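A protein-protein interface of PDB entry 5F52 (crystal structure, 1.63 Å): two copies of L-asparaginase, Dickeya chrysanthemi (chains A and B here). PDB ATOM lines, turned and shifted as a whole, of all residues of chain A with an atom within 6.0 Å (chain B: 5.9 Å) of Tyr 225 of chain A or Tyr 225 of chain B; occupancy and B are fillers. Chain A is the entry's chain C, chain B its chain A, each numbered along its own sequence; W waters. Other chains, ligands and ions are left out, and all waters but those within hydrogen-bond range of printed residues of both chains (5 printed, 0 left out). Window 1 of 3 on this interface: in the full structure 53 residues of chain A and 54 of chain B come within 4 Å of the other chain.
N of Ile 223 of chain B is in hydrogen-bond range of OH of Tyr 227 of chain A (3.0 Å). OH of Tyr 227 of chain B sits at hydrogen-bond distance from N of Ile 223 of chain A.
Hydrophobic or aromatic side chains of chain B within 4 Å of the printed part of chain A: Ile 223, Tyr 225, Tyr 227, Pro 301 and Ala 302. Along chain B the printed residues that touch a printed residue of chain A span positions 223 to 302. Hydrophobic or aromatic side chains of chain A within 4 Å of the printed part of chain B: Ile 223, Tyr 225, Tyr 227, Pro 301 and Ala 302. Among the printed residues, 9 pairs touch across the chains. Among the printed residues, no Asp or Glu carboxylate lies within 4 Å of a Lys or Arg side-chain nitrogen of the other chain.
Of chain B, only Ile 223, Tyr 225 and Pro 301 come within 4 Å of Tyr 225 of chain A. Tyr 225 of chain B touches just these residues of chain A: Ile 223, Tyr 225 and Pro 301. Of the printed residues of chain A, Arg 279 of chain B touches Ala 302. Printed residues of chain B within 4 Å of Ile 223 of chain A: Tyr 225 and Tyr 227. Of the printed residues of chain A, Ala 302 of chain B touches Arg 279 (3.9 Å). Of the printed residues of chain B, Ala 302 of chain A touches Arg 279 (3.9 Å). The nearest residue of chain B that does not touch Tyr 225 of chain A is Ala 249 of chain B (4.5 Å).
Water W4 lies within hydrogen-bond range of OH of Tyr 225 of chain A (2.6 Å) and N of Ala 302 of chain B (2.9 Å). Water W2 lies within hydrogen-bond range of OH of Tyr 225 of chain B (2.7 Å) and N of Ala 302 of chain A (2.9 Å). Water W1 bridges O of Ile 223 of chain B and N of Tyr 225 of chain A. Water W5 lies within hydrogen-bond range of O of Ile 223 of chain A (2.7 Å) and N of Tyr 225 of chain B (2.9 Å). Water W3 bridges the backbone carbonyl oxygen of Arg 279 of chain B and the backbone carbonyl oxygen of Arg 279 of chain A.
The guanidinium group of Arg 279 of chain B lies within hydrogen-bond range of the backbone carbonyl oxygen of Gly 226 of chain B (2.9 Å). The backbone carbonyl oxygen of Gly 250 of chain B is in hydrogen-bond range of the backbone NH of Arg 279 of chain B (2.8 Å). The backbone carbonyl oxygen of Gly 226 of chain A is in hydrogen-bond range of the guanidinium group of Arg 279 of chain A. The backbone carbonyl oxygen (O) of Gly 250 of chain A lies within hydrogen-bond range of the backbone NH (N) of Arg 279 of chain A, at 2.8 Å.
Ile 223 of chain A touches Tyr 225 of chain B, and with the chains exchanged Tyr 225 of chain A touches Ile 223 of chain B. Ile 223 of chain A touches Tyr 227 of chain B, and with the chains exchanged Tyr 227 of chain A touches Ile 223 of chain B. Tyr 225 of chain A touches its own counterpart, Tyr 225 of chain B. Tyr 225 of chain A touches Pro 301 of chain B, and with the chains exchanged Pro 301 of chain A touches Tyr 225 of chain B. Of the 9 pairs that touch across the chains among the printed residues, 9 have their exchanged pair printed and touching as well.
Among the printed residues, pairs that only touch across the chains: Ile 223 of chain A with Tyr 225 of chain B, Tyr 225 of chain A with Ile 223 of chain B, Tyr 225 of chain A with Tyr 225 of chain B, Tyr 225 of chain A with Pro 301 of chain B, Arg 279 of chain A with Ala 302 of chain B, Pro 301 of chain A with Tyr 225 of chain B and Ala 302 of chain A with Arg 279 of chain B.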
ATOM      1  N   ILE A 223      -8.666  32.962  31.292  1.00  0.00           N
ATOM      2  CA  ILE A 223      -8.896  32.013  30.231  1.00  0.00           C
ATOM      3  C   ILE A 223     -10.333  32.063  29.793  1.00  0.00           C
ATOM      4  O   ILE A 223     -11.232  32.015  30.628  1.00  0.00           O
ATOM      5  CB  ILE A 223      -8.602  30.563  30.704  1.00  0.00           C
ATOM      6  CG1 ILE A 223      -7.175  30.438  31.234  1.00  0.00           C
ATOM      7  CG2 ILE A 223      -8.886  29.576  29.580  1.00  0.00           C
ATOM      8  CD1 ILE A 223      -6.842  29.073  31.803  1.00  0.00           C
ATOM      9  N   LEU A 224     -10.560  32.193  28.498  1.00  0.00           N
ATOM     10  CA  LEU A 224     -11.850  32.318  27.907  1.00  0.00           C
ATOM     11  C   LEU A 224     -12.046  31.136  26.961  1.00  0.00           C
ATOM     12  O   LEU A 224     -11.148  30.787  26.171  1.00  0.00           O
ATOM     13  CB  LEU A 224     -12.025  33.628  27.128  1.00  0.00           C
ATOM     14  CG  LEU A 224     -11.924  34.888  27.987  1.00  0.00           C
ATOM     15  CD1 LEU A 224     -12.144  36.126  27.102  1.00  0.00           C
ATOM     16  CD2 LEU A 224     -12.933  34.863  29.091  1.00  0.00           C
ATOM     17  N   TYR A 225     -13.255  30.586  27.014  1.00  0.00           N
ATOM     18  CA  TYR A 225     -13.546  29.393  26.250  1.00  0.00           C
ATOM     19  C   TYR A 225     -14.019  29.784  24.851  1.00  0.00           C
ATOM     20  O   TYR A 225     -14.674  30.840  24.673  1.00  0.00           O
ATOM     21  CB  TYR A 225     -14.626  28.608  26.944  1.00  0.00           C
ATOM     22  CG  TYR A 225     -14.610  27.120  26.708  1.00  0.00           C
ATOM     23  CD1 TYR A 225     -13.591  26.345  27.235  1.00  0.00           C
ATOM     24  CD2 TYR A 225     -15.615  26.474  26.003  1.00  0.00           C
ATOM     25  CE1 TYR A 225     -13.547  24.990  27.029  1.00  0.00           C
ATOM     26  CE2 TYR A 225     -15.594  25.089  25.858  1.00  0.00           C
ATOM     27  CZ  TYR A 225     -14.562  24.369  26.415  1.00  0.00           C
ATOM     28  OH  TYR A 225     -14.561  22.965  26.276  1.00  0.00           O
ATOM     29  N   GLY A 226     -13.730  28.942  23.854  1.00  0.00           N
ATOM     30  CA  GLY A 226     -14.293  29.111  22.544  1.00  0.00           C
ATOM     31  C   GLY A 226     -15.373  28.062  22.251  1.00  0.00           C
ATOM     32  O   GLY A 226     -15.252  26.878  22.577  1.00  0.00           O
ATOM     33  N   TYR A 227     -16.447  28.518  21.639  1.00  0.00           N
ATOM     34  CA  TYR A 227     -17.615  27.718  21.391  1.00  0.00           C
ATOM     35  C   TYR A 227     -18.557  28.469  20.433  1.00  0.00           C
ATOM     36  O   TYR A 227     -18.424  29.665  20.275  1.00  0.00           O
ATOM     37  CB  TYR A 227     -18.350  27.355  22.701  1.00  0.00           C
ATOM     38  CG  TYR A 227     -18.725  28.506  23.608  1.00  0.00           C
ATOM     39  CD1 TYR A 227     -17.800  29.094  24.461  1.00  0.00           C
ATOM     40  CD2 TYR A 227     -20.048  28.962  23.673  1.00  0.00           C
ATOM     41  CE1 TYR A 227     -18.141  30.156  25.271  1.00  0.00           C
ATOM     42  CE2 TYR A 227     -20.394  29.948  24.541  1.00  0.00           C
ATOM     43  CZ  TYR A 227     -19.464  30.547  25.342  1.00  0.00           C
ATOM     44  OH  TYR A 227     -19.768  31.556  26.226  1.00  0.00           O
ATOM     45  N   ASP A 230     -19.893  32.193  21.111  1.00  0.00           N
ATOM     46  CA  ASP A 230     -19.108  32.735  22.164  1.00  0.00           C
ATOM     47  C   ASP A 230     -19.214  34.284  22.169  1.00  0.00           C
ATOM     48  O   ASP A 230     -19.155  34.899  21.124  1.00  0.00           O
ATOM     49  CB  ASP A 230     -17.667  32.265  22.112  1.00  0.00           C
ATOM     50  CG  ASP A 230     -16.953  32.613  20.814  1.00  0.00           C
ATOM     51  OD1 ASP A 230     -17.580  32.911  19.745  1.00  0.00           O
ATOM     52  OD2 ASP A 230     -15.737  32.554  20.862  1.00  0.00           O
ATOM     53  N   PRO A 231     -19.365  34.879  23.351  1.00  0.00           N
ATOM     54  CA  PRO A 231     -19.638  36.310  23.367  1.00  0.00           C
ATOM     55  C   PRO A 231     -18.432  37.229  23.499  1.00  0.00           C
ATOM     56  O   PRO A 231     -17.480  36.980  24.214  1.00  0.00           O
ATOM     57  CB  PRO A 231     -20.507  36.459  24.585  1.00  0.00           C
ATOM     58  CG  PRO A 231     -19.889  35.489  25.534  1.00  0.00           C
ATOM     59  CD  PRO A 231     -19.533  34.289  24.676  1.00  0.00           C
ATOM     60  N   TYR A 235     -14.514  39.274  26.712  1.00  0.00           N
ATOM     61  CA  TYR A 235     -13.253  39.962  26.402  1.00  0.00           C
ATOM     62  C   TYR A 235     -13.330  41.357  26.964  1.00  0.00           C
ATOM     63  O   TYR A 235     -12.411  41.767  27.671  1.00  0.00           O
ATOM     64  CB  TYR A 235     -12.970  40.036  24.894  1.00  0.00           C
ATOM     65  CG  TYR A 235     -12.701  38.689  24.275  1.00  0.00           C
ATOM     66  CD1 TYR A 235     -13.762  37.855  23.869  1.00  0.00           C
ATOM     67  CD2 TYR A 235     -11.419  38.221  24.155  1.00  0.00           C
ATOM     68  CE1 TYR A 235     -13.531  36.590  23.322  1.00  0.00           C
ATOM     69  CE2 TYR A 235     -11.197  36.977  23.576  1.00  0.00           C
ATOM     70  CZ  TYR A 235     -12.236  36.183  23.169  1.00  0.00           C
ATOM     71  OH  TYR A 235     -11.990  34.924  22.697  1.00  0.00           O
ATOM     72  N   VAL A 247      -5.717  33.790  27.709  1.00  0.00           N
ATOM     73  CA  VAL A 247      -5.567  32.512  27.016  1.00  0.00           C
ATOM     74  C   VAL A 247      -6.913  32.120  26.504  1.00  0.00           C
ATOM     75  O   VAL A 247      -7.872  32.076  27.215  1.00  0.00           O
ATOM     76  CB  VAL A 247      -4.973  31.432  27.951  1.00  0.00           C
ATOM     77  CG1 VAL A 247      -4.980  30.082  27.268  1.00  0.00           C
ATOM     78  CG2 VAL A 247      -3.557  31.813  28.375  1.00  0.00           C
ATOM     79  N   TYR A 248      -6.958  31.815  25.207  1.00  0.00           N
ATOM     80  CA  TYR A 248      -8.235  31.422  24.547  1.00  0.00           C
ATOM     81  C   TYR A 248      -8.219  29.912  24.384  1.00  0.00           C
ATOM     82  O   TYR A 248      -7.302  29.360  23.736  1.00  0.00           O
ATOM     83  CB  TYR A 248      -8.276  32.128  23.197  1.00  0.00           C
ATOM     84  CG  TYR A 248      -9.335  31.690  22.273  1.00  0.00           C
ATOM     85  CD1 TYR A 248     -10.679  31.828  22.612  1.00  0.00           C
ATOM     86  CD2 TYR A 248      -9.011  31.137  21.016  1.00  0.00           C
ATOM     87  CE1 TYR A 248     -11.688  31.409  21.740  1.00  0.00           C
ATOM     88  CE2 TYR A 248      -9.986  30.756  20.156  1.00  0.00           C
ATOM     89  CZ  TYR A 248     -11.310  30.853  20.528  1.00  0.00           C
ATOM     90  OH  TYR A 248     -12.271  30.397  19.651  1.00  0.00           O
ATOM     91  N   ALA A 249      -9.165  29.246  24.994  1.00  0.00           N
ATOM     92  CA  ALA A 249      -9.290  27.780  24.888  1.00  0.00           C
ATOM     93  C   ALA A 249     -10.149  27.544  23.662  1.00  0.00           C
ATOM     94  O   ALA A 249     -11.378  27.379  23.753  1.00  0.00           O
ATOM     95  CB  ALA A 249      -9.900  27.195  26.162  1.00  0.00           C
ATOM     96  N   GLY A 250      -9.498  27.591  22.514  1.00  0.00           N
ATOM     97  CA  GLY A 250     -10.175  27.736  21.255  1.00  0.00           C
ATOM     98  C   GLY A 250     -10.855  26.504  20.684  1.00  0.00           C
ATOM     99  O   GLY A 250     -10.536  25.380  21.045  1.00  0.00           O
ATOM    100  N   THR A 278      -6.243  25.548  22.729  1.00  0.00           N
ATOM    101  CA  THR A 278      -7.319  24.700  22.253  1.00  0.00           C
ATOM    102  C   THR A 278      -8.115  24.094  23.359  1.00  0.00           C
ATOM    103  O   THR A 278      -7.565  23.793  24.333  1.00  0.00           O
ATOM    104  CB  THR A 278      -6.737  23.548  21.368  1.00  0.00           C
ATOM    105  OG1 THR A 278      -7.743  22.677  20.924  1.00  0.00           O
ATOM    106  CG2 THR A 278      -5.635  22.736  22.065  1.00  0.00           C
ATOM    107  N   ARG A 279      -9.410  23.926  23.160  1.00  0.00           N
ATOM    108  CA  ARG A 279     -10.229  23.262  24.159  1.00  0.00           C
ATOM    109  C   ARG A 279     -10.181  21.753  23.954  1.00  0.00           C
ATOM    110  O   ARG A 279     -10.795  21.034  24.692  1.00  0.00           O
ATOM    111  CB  ARG A 279     -11.698  23.772  24.029  1.00  0.00           C
ATOM    112  CG  ARG A 279     -12.470  23.206  22.812  1.00  0.00           C
ATOM    113  CD  ARG A 279     -13.846  23.856  22.590  1.00  0.00           C
ATOM    114  NE  ARG A 279     -14.534  23.163  21.500  1.00  0.00           N
ATOM    115  CZ  ARG A 279     -15.771  23.444  21.079  1.00  0.00           C
ATOM    116  NH1 ARG A 279     -16.461  24.405  21.687  1.00  0.00           N
ATOM    117  NH2 ARG A 279     -16.367  22.649  20.168  1.00  0.00           N
ATOM    118  N   PRO A 301      -4.794  24.918  27.780  1.00  0.00           N
ATOM    119  CA  PRO A 301      -5.063  26.245  28.296  1.00  0.00           C
ATOM    120  C   PRO A 301      -4.519  26.515  29.669  1.00  0.00           C
ATOM    121  O   PRO A 301      -3.963  27.631  29.916  1.00  0.00           O
ATOM    122  CB  PRO A 301      -6.588  26.304  28.260  1.00  0.00           C
ATOM    123  CG  PRO A 301      -6.952  25.494  27.093  1.00  0.00           C
ATOM    124  CD  PRO A 301      -6.011  24.329  27.203  1.00  0.00           C
ATOM    125  N   ALA A 302      -4.623  25.544  30.569  1.00  0.00           N
ATOM    126  CA  ALA A 302      -4.145  25.741  31.961  1.00  0.00           C
ATOM    127  C   ALA A 302      -2.630  25.960  31.993  1.00  0.00           C
ATOM    128  O   ALA A 302      -2.126  26.853  32.686  1.00  0.00           O
ATOM    129  CB  ALA A 302      -4.510  24.524  32.765  1.00  0.00           C
ATOM    130  N   ILE B 223     -20.218  29.639  28.535  1.00  0.00           N
ATOM    131  CA  ILE B 223     -19.319  28.629  29.176  1.00  0.00           C
ATOM    132  C   ILE B 223     -18.166  29.379  29.811  1.00  0.00           C
ATOM    133  O   ILE B 223     -17.542  30.185  29.168  1.00  0.00           O
ATOM    134  CB  ILE B 223     -18.779  27.635  28.153  1.00  0.00           C
ATOM    135  CG1 ILE B 223     -19.931  26.931  27.443  1.00  0.00           C
ATOM    136  CG2 ILE B 223     -17.816  26.666  28.834  1.00  0.00           C
ATOM    137  CD1 ILE B 223     -19.468  25.987  26.383  1.00  0.00           C
ATOM    138  N   LEU B 224     -17.890  29.094  31.104  1.00  0.00           N
ATOM    139  CA  LEU B 224     -16.828  29.731  31.849  1.00  0.00           C
ATOM    140  C   LEU B 224     -15.867  28.661  32.321  1.00  0.00           C
ATOM    141  O   LEU B 224     -16.295  27.572  32.756  1.00  0.00           O
ATOM    142  CB  LEU B 224     -17.399  30.457  33.094  1.00  0.00           C
ATOM    143  CG  LEU B 224     -18.338  31.633  32.758  1.00  0.00           C
ATOM    144  CD1 LEU B 224     -18.768  32.254  34.054  1.00  0.00           C
ATOM    145  CD2 LEU B 224     -17.668  32.660  31.850  1.00  0.00           C
ATOM    146  N   TYR B 225     -14.580  28.948  32.142  1.00  0.00           N
ATOM    147  CA  TYR B 225     -13.548  27.993  32.454  1.00  0.00           C
ATOM    148  C   TYR B 225     -13.204  28.045  33.917  1.00  0.00           C
ATOM    149  O   TYR B 225     -13.284  29.100  34.579  1.00  0.00           O
ATOM    150  CB  TYR B 225     -12.314  28.310  31.653  1.00  0.00           C
ATOM    151  CG  TYR B 225     -11.452  27.171  31.268  1.00  0.00           C
ATOM    152  CD1 TYR B 225     -11.896  26.236  30.344  1.00  0.00           C
ATOM    153  CD2 TYR B 225     -10.160  27.069  31.709  1.00  0.00           C
ATOM    154  CE1 TYR B 225     -11.109  25.191  29.942  1.00  0.00           C
ATOM    155  CE2 TYR B 225      -9.379  25.984  31.336  1.00  0.00           C
ATOM    156  CZ  TYR B 225      -9.837  25.099  30.421  1.00  0.00           C
ATOM    157  OH  TYR B 225      -9.025  24.053  30.022  1.00  0.00           O
ATOM    158  N   GLY B 226     -12.794  26.894  34.459  1.00  0.00           N
ATOM    159  CA  GLY B 226     -12.298  26.793  35.805  1.00  0.00           C
ATOM    160  C   GLY B 226     -10.779  26.609  35.779  1.00  0.00           C
ATOM    161  O   GLY B 226     -10.237  25.810  35.033  1.00  0.00           O
ATOM    162  N   TYR B 227     -10.104  27.344  36.654  1.00  0.00           N
ATOM    163  CA  TYR B 227      -8.643  27.330  36.731  1.00  0.00           C
ATOM    164  C   TYR B 227      -8.204  28.102  37.977  1.00  0.00           C
ATOM    165  O   TYR B 227      -9.018  28.742  38.626  1.00  0.00           O
ATOM    166  CB  TYR B 227      -8.033  27.950  35.495  1.00  0.00           C
ATOM    167  CG  TYR B 227      -8.543  29.376  35.156  1.00  0.00           C
ATOM    168  CD1 TYR B 227      -9.735  29.586  34.551  1.00  0.00           C
ATOM    169  CD2 TYR B 227      -7.769  30.502  35.472  1.00  0.00           C
ATOM    170  CE1 TYR B 227     -10.150  30.868  34.189  1.00  0.00           C
ATOM    171  CE2 TYR B 227      -8.210  31.785  35.146  1.00  0.00           C
ATOM    172  CZ  TYR B 227      -9.398  31.930  34.509  1.00  0.00           C
ATOM    173  OH  TYR B 227      -9.862  33.172  34.101  1.00  0.00           O
ATOM    174  N   ASP B 230      -9.385  31.736  39.058  1.00  0.00           N
ATOM    175  CA  ASP B 230     -10.518  32.075  38.195  1.00  0.00           C
ATOM    176  C   ASP B 230     -11.365  33.217  38.801  1.00  0.00           C
ATOM    177  O   ASP B 230     -11.609  33.206  39.991  1.00  0.00           O
ATOM    178  CB  ASP B 230     -11.377  30.850  37.886  1.00  0.00           C
ATOM    179  CG  ASP B 230     -11.992  30.195  39.106  1.00  0.00           C
ATOM    180  OD1 ASP B 230     -11.539  30.333  40.260  1.00  0.00           O
ATOM    181  OD2 ASP B 230     -12.939  29.445  38.855  1.00  0.00           O
ATOM    182  N   TYR B 235     -18.557  35.705  35.967  1.00  0.00           N
ATOM    183  CA  TYR B 235     -19.940  35.363  36.336  1.00  0.00           C
ATOM    184  C   TYR B 235     -20.803  36.627  36.347  1.00  0.00           C
ATOM    185  O   TYR B 235     -21.899  36.630  35.792  1.00  0.00           O
ATOM    186  CB  TYR B 235     -20.063  34.673  37.700  1.00  0.00           C
ATOM    187  CG  TYR B 235     -19.397  33.302  37.711  1.00  0.00           C
ATOM    188  CD1 TYR B 235     -18.024  33.189  37.868  1.00  0.00           C
ATOM    189  CD2 TYR B 235     -20.135  32.185  37.489  1.00  0.00           C
ATOM    190  CE1 TYR B 235     -17.402  31.936  37.834  1.00  0.00           C
ATOM    191  CE2 TYR B 235     -19.518  30.927  37.431  1.00  0.00           C
ATOM    192  CZ  TYR B 235     -18.157  30.841  37.633  1.00  0.00           C
ATOM    193  OH  TYR B 235     -17.580  29.603  37.591  1.00  0.00           O
ATOM    194  N   VAL B 247     -22.635  27.072  31.772  1.00  0.00           N
ATOM    195  CA  VAL B 247     -21.906  25.787  31.880  1.00  0.00           C
ATOM    196  C   VAL B 247     -20.493  26.073  32.356  1.00  0.00           C
ATOM    197  O   VAL B 247     -19.804  26.970  31.848  1.00  0.00           O
ATOM    198  CB  VAL B 247     -21.844  25.080  30.534  1.00  0.00           C
ATOM    199  CG1 VAL B 247     -20.943  23.850  30.661  1.00  0.00           C
ATOM    200  CG2 VAL B 247     -23.214  24.667  30.095  1.00  0.00           C
ATOM    201  N   TYR B 248     -20.078  25.428  33.433  1.00  0.00           N
ATOM    202  CA  TYR B 248     -18.814  25.643  34.069  1.00  0.00           C
ATOM    203  C   TYR B 248     -17.910  24.507  33.649  1.00  0.00           C
ATOM    204  O   TYR B 248     -18.213  23.344  33.902  1.00  0.00           O
ATOM    205  CB  TYR B 248     -19.017  25.644  35.560  1.00  0.00           C
ATOM    206  CG  TYR B 248     -17.757  25.584  36.354  1.00  0.00           C
ATOM    207  CD1 TYR B 248     -16.810  26.613  36.298  1.00  0.00           C
ATOM    208  CD2 TYR B 248     -17.492  24.500  37.214  1.00  0.00           C
ATOM    209  CE1 TYR B 248     -15.650  26.586  37.075  1.00  0.00           C
ATOM    210  CE2 TYR B 248     -16.404  24.528  38.026  1.00  0.00           C
ATOM    211  CZ  TYR B 248     -15.457  25.527  37.920  1.00  0.00           C
ATOM    212  OH  TYR B 248     -14.306  25.402  38.667  1.00  0.00           O
ATOM    213  N   ALA B 249     -16.820  24.845  32.975  1.00  0.00           N
ATOM    214  CA  ALA B 249     -15.838  23.834  32.507  1.00  0.00           C
ATOM    215  C   ALA B 249     -14.825  23.686  33.622  1.00  0.00           C
ATOM    216  O   ALA B 249     -13.794  24.341  33.627  1.00  0.00           O
ATOM    217  CB  ALA B 249     -15.195  24.288  31.206  1.00  0.00           C
ATOM    218  N   GLY B 250     -15.232  22.904  34.597  1.00  0.00           N
ATOM    219  CA  GLY B 250     -14.649  22.897  35.890  1.00  0.00           C
ATOM    220  C   GLY B 250     -13.286  22.238  35.992  1.00  0.00           C
ATOM    221  O   GLY B 250     -12.927  21.375  35.203  1.00  0.00           O
ATOM    222  N   THR B 278     -16.705  19.648  33.208  1.00  0.00           N
ATOM    223  CA  THR B 278     -15.249  19.476  33.447  1.00  0.00           C
ATOM    224  C   THR B 278     -14.428  19.971  32.281  1.00  0.00           C
ATOM    225  O   THR B 278     -14.842  19.796  31.135  1.00  0.00           O
ATOM    226  CB  THR B 278     -14.936  18.007  33.790  1.00  0.00           C
ATOM    227  OG1 THR B 278     -13.547  17.806  33.986  1.00  0.00           O
ATOM    228  CG2 THR B 278     -15.374  16.988  32.650  1.00  0.00           C
ATOM    229  N   ARG B 279     -13.274  20.560  32.541  1.00  0.00           N
ATOM    230  CA  ARG B 279     -12.335  20.943  31.493  1.00  0.00           C
ATOM    231  C   ARG B 279     -11.461  19.743  31.120  1.00  0.00           C
ATOM    232  O   ARG B 279     -10.623  19.850  30.226  1.00  0.00           O
ATOM    233  CB  ARG B 279     -11.415  22.070  31.980  1.00  0.00           C
ATOM    234  CG  ARG B 279     -10.357  21.669  33.000  1.00  0.00           C
ATOM    235  CD  ARG B 279      -9.627  22.848  33.648  1.00  0.00           C
ATOM    236  NE  ARG B 279      -8.475  22.370  34.392  1.00  0.00           N
ATOM    237  CZ  ARG B 279      -7.586  23.128  35.016  1.00  0.00           C
ATOM    238  NH1 ARG B 279      -7.721  24.410  35.029  1.00  0.00           N
ATOM    239  NH2 ARG B 279      -6.532  22.539  35.675  1.00  0.00           N
ATOM    240  N   PRO B 301     -18.163  20.314  28.105  1.00  0.00           N
ATOM    241  CA  PRO B 301     -18.818  21.593  28.221  1.00  0.00           C
ATOM    242  C   PRO B 301     -19.587  22.012  26.997  1.00  0.00           C
ATOM    243  O   PRO B 301     -20.660  22.554  27.125  1.00  0.00           O
ATOM    244  CB  PRO B 301     -17.611  22.553  28.471  1.00  0.00           C
ATOM    245  CG  PRO B 301     -16.672  21.724  29.301  1.00  0.00           C
ATOM    246  CD  PRO B 301     -16.770  20.382  28.609  1.00  0.00           C
ATOM    247  N   ALA B 302     -19.011  21.755  25.821  1.00  0.00           N
ATOM    248  CA  ALA B 302     -19.679  22.118  24.558  1.00  0.00           C
ATOM    249  C   ALA B 302     -21.025  21.380  24.384  1.00  0.00           C
ATOM    250  O   ALA B 302     -22.037  21.998  24.021  1.00  0.00           O
ATOM    251  CB  ALA B 302     -18.760  21.795  23.402  1.00  0.00           C
HETATM  252  O   HOH W   1     -15.291  31.657  28.751  1.00  0.00           O
HETATM  253  O   HOH W   2      -6.448  23.340  30.438  1.00  0.00           O
HETATM  254  O   HOH W   3     -10.222  18.852  27.219  1.00  0.00           O
HETATM  255  O   HOH W   4     -16.177  21.084  25.383  1.00  0.00           O
HETATM  256  O   HOH W   5     -13.883  31.570  31.197  1.00  0.00           O
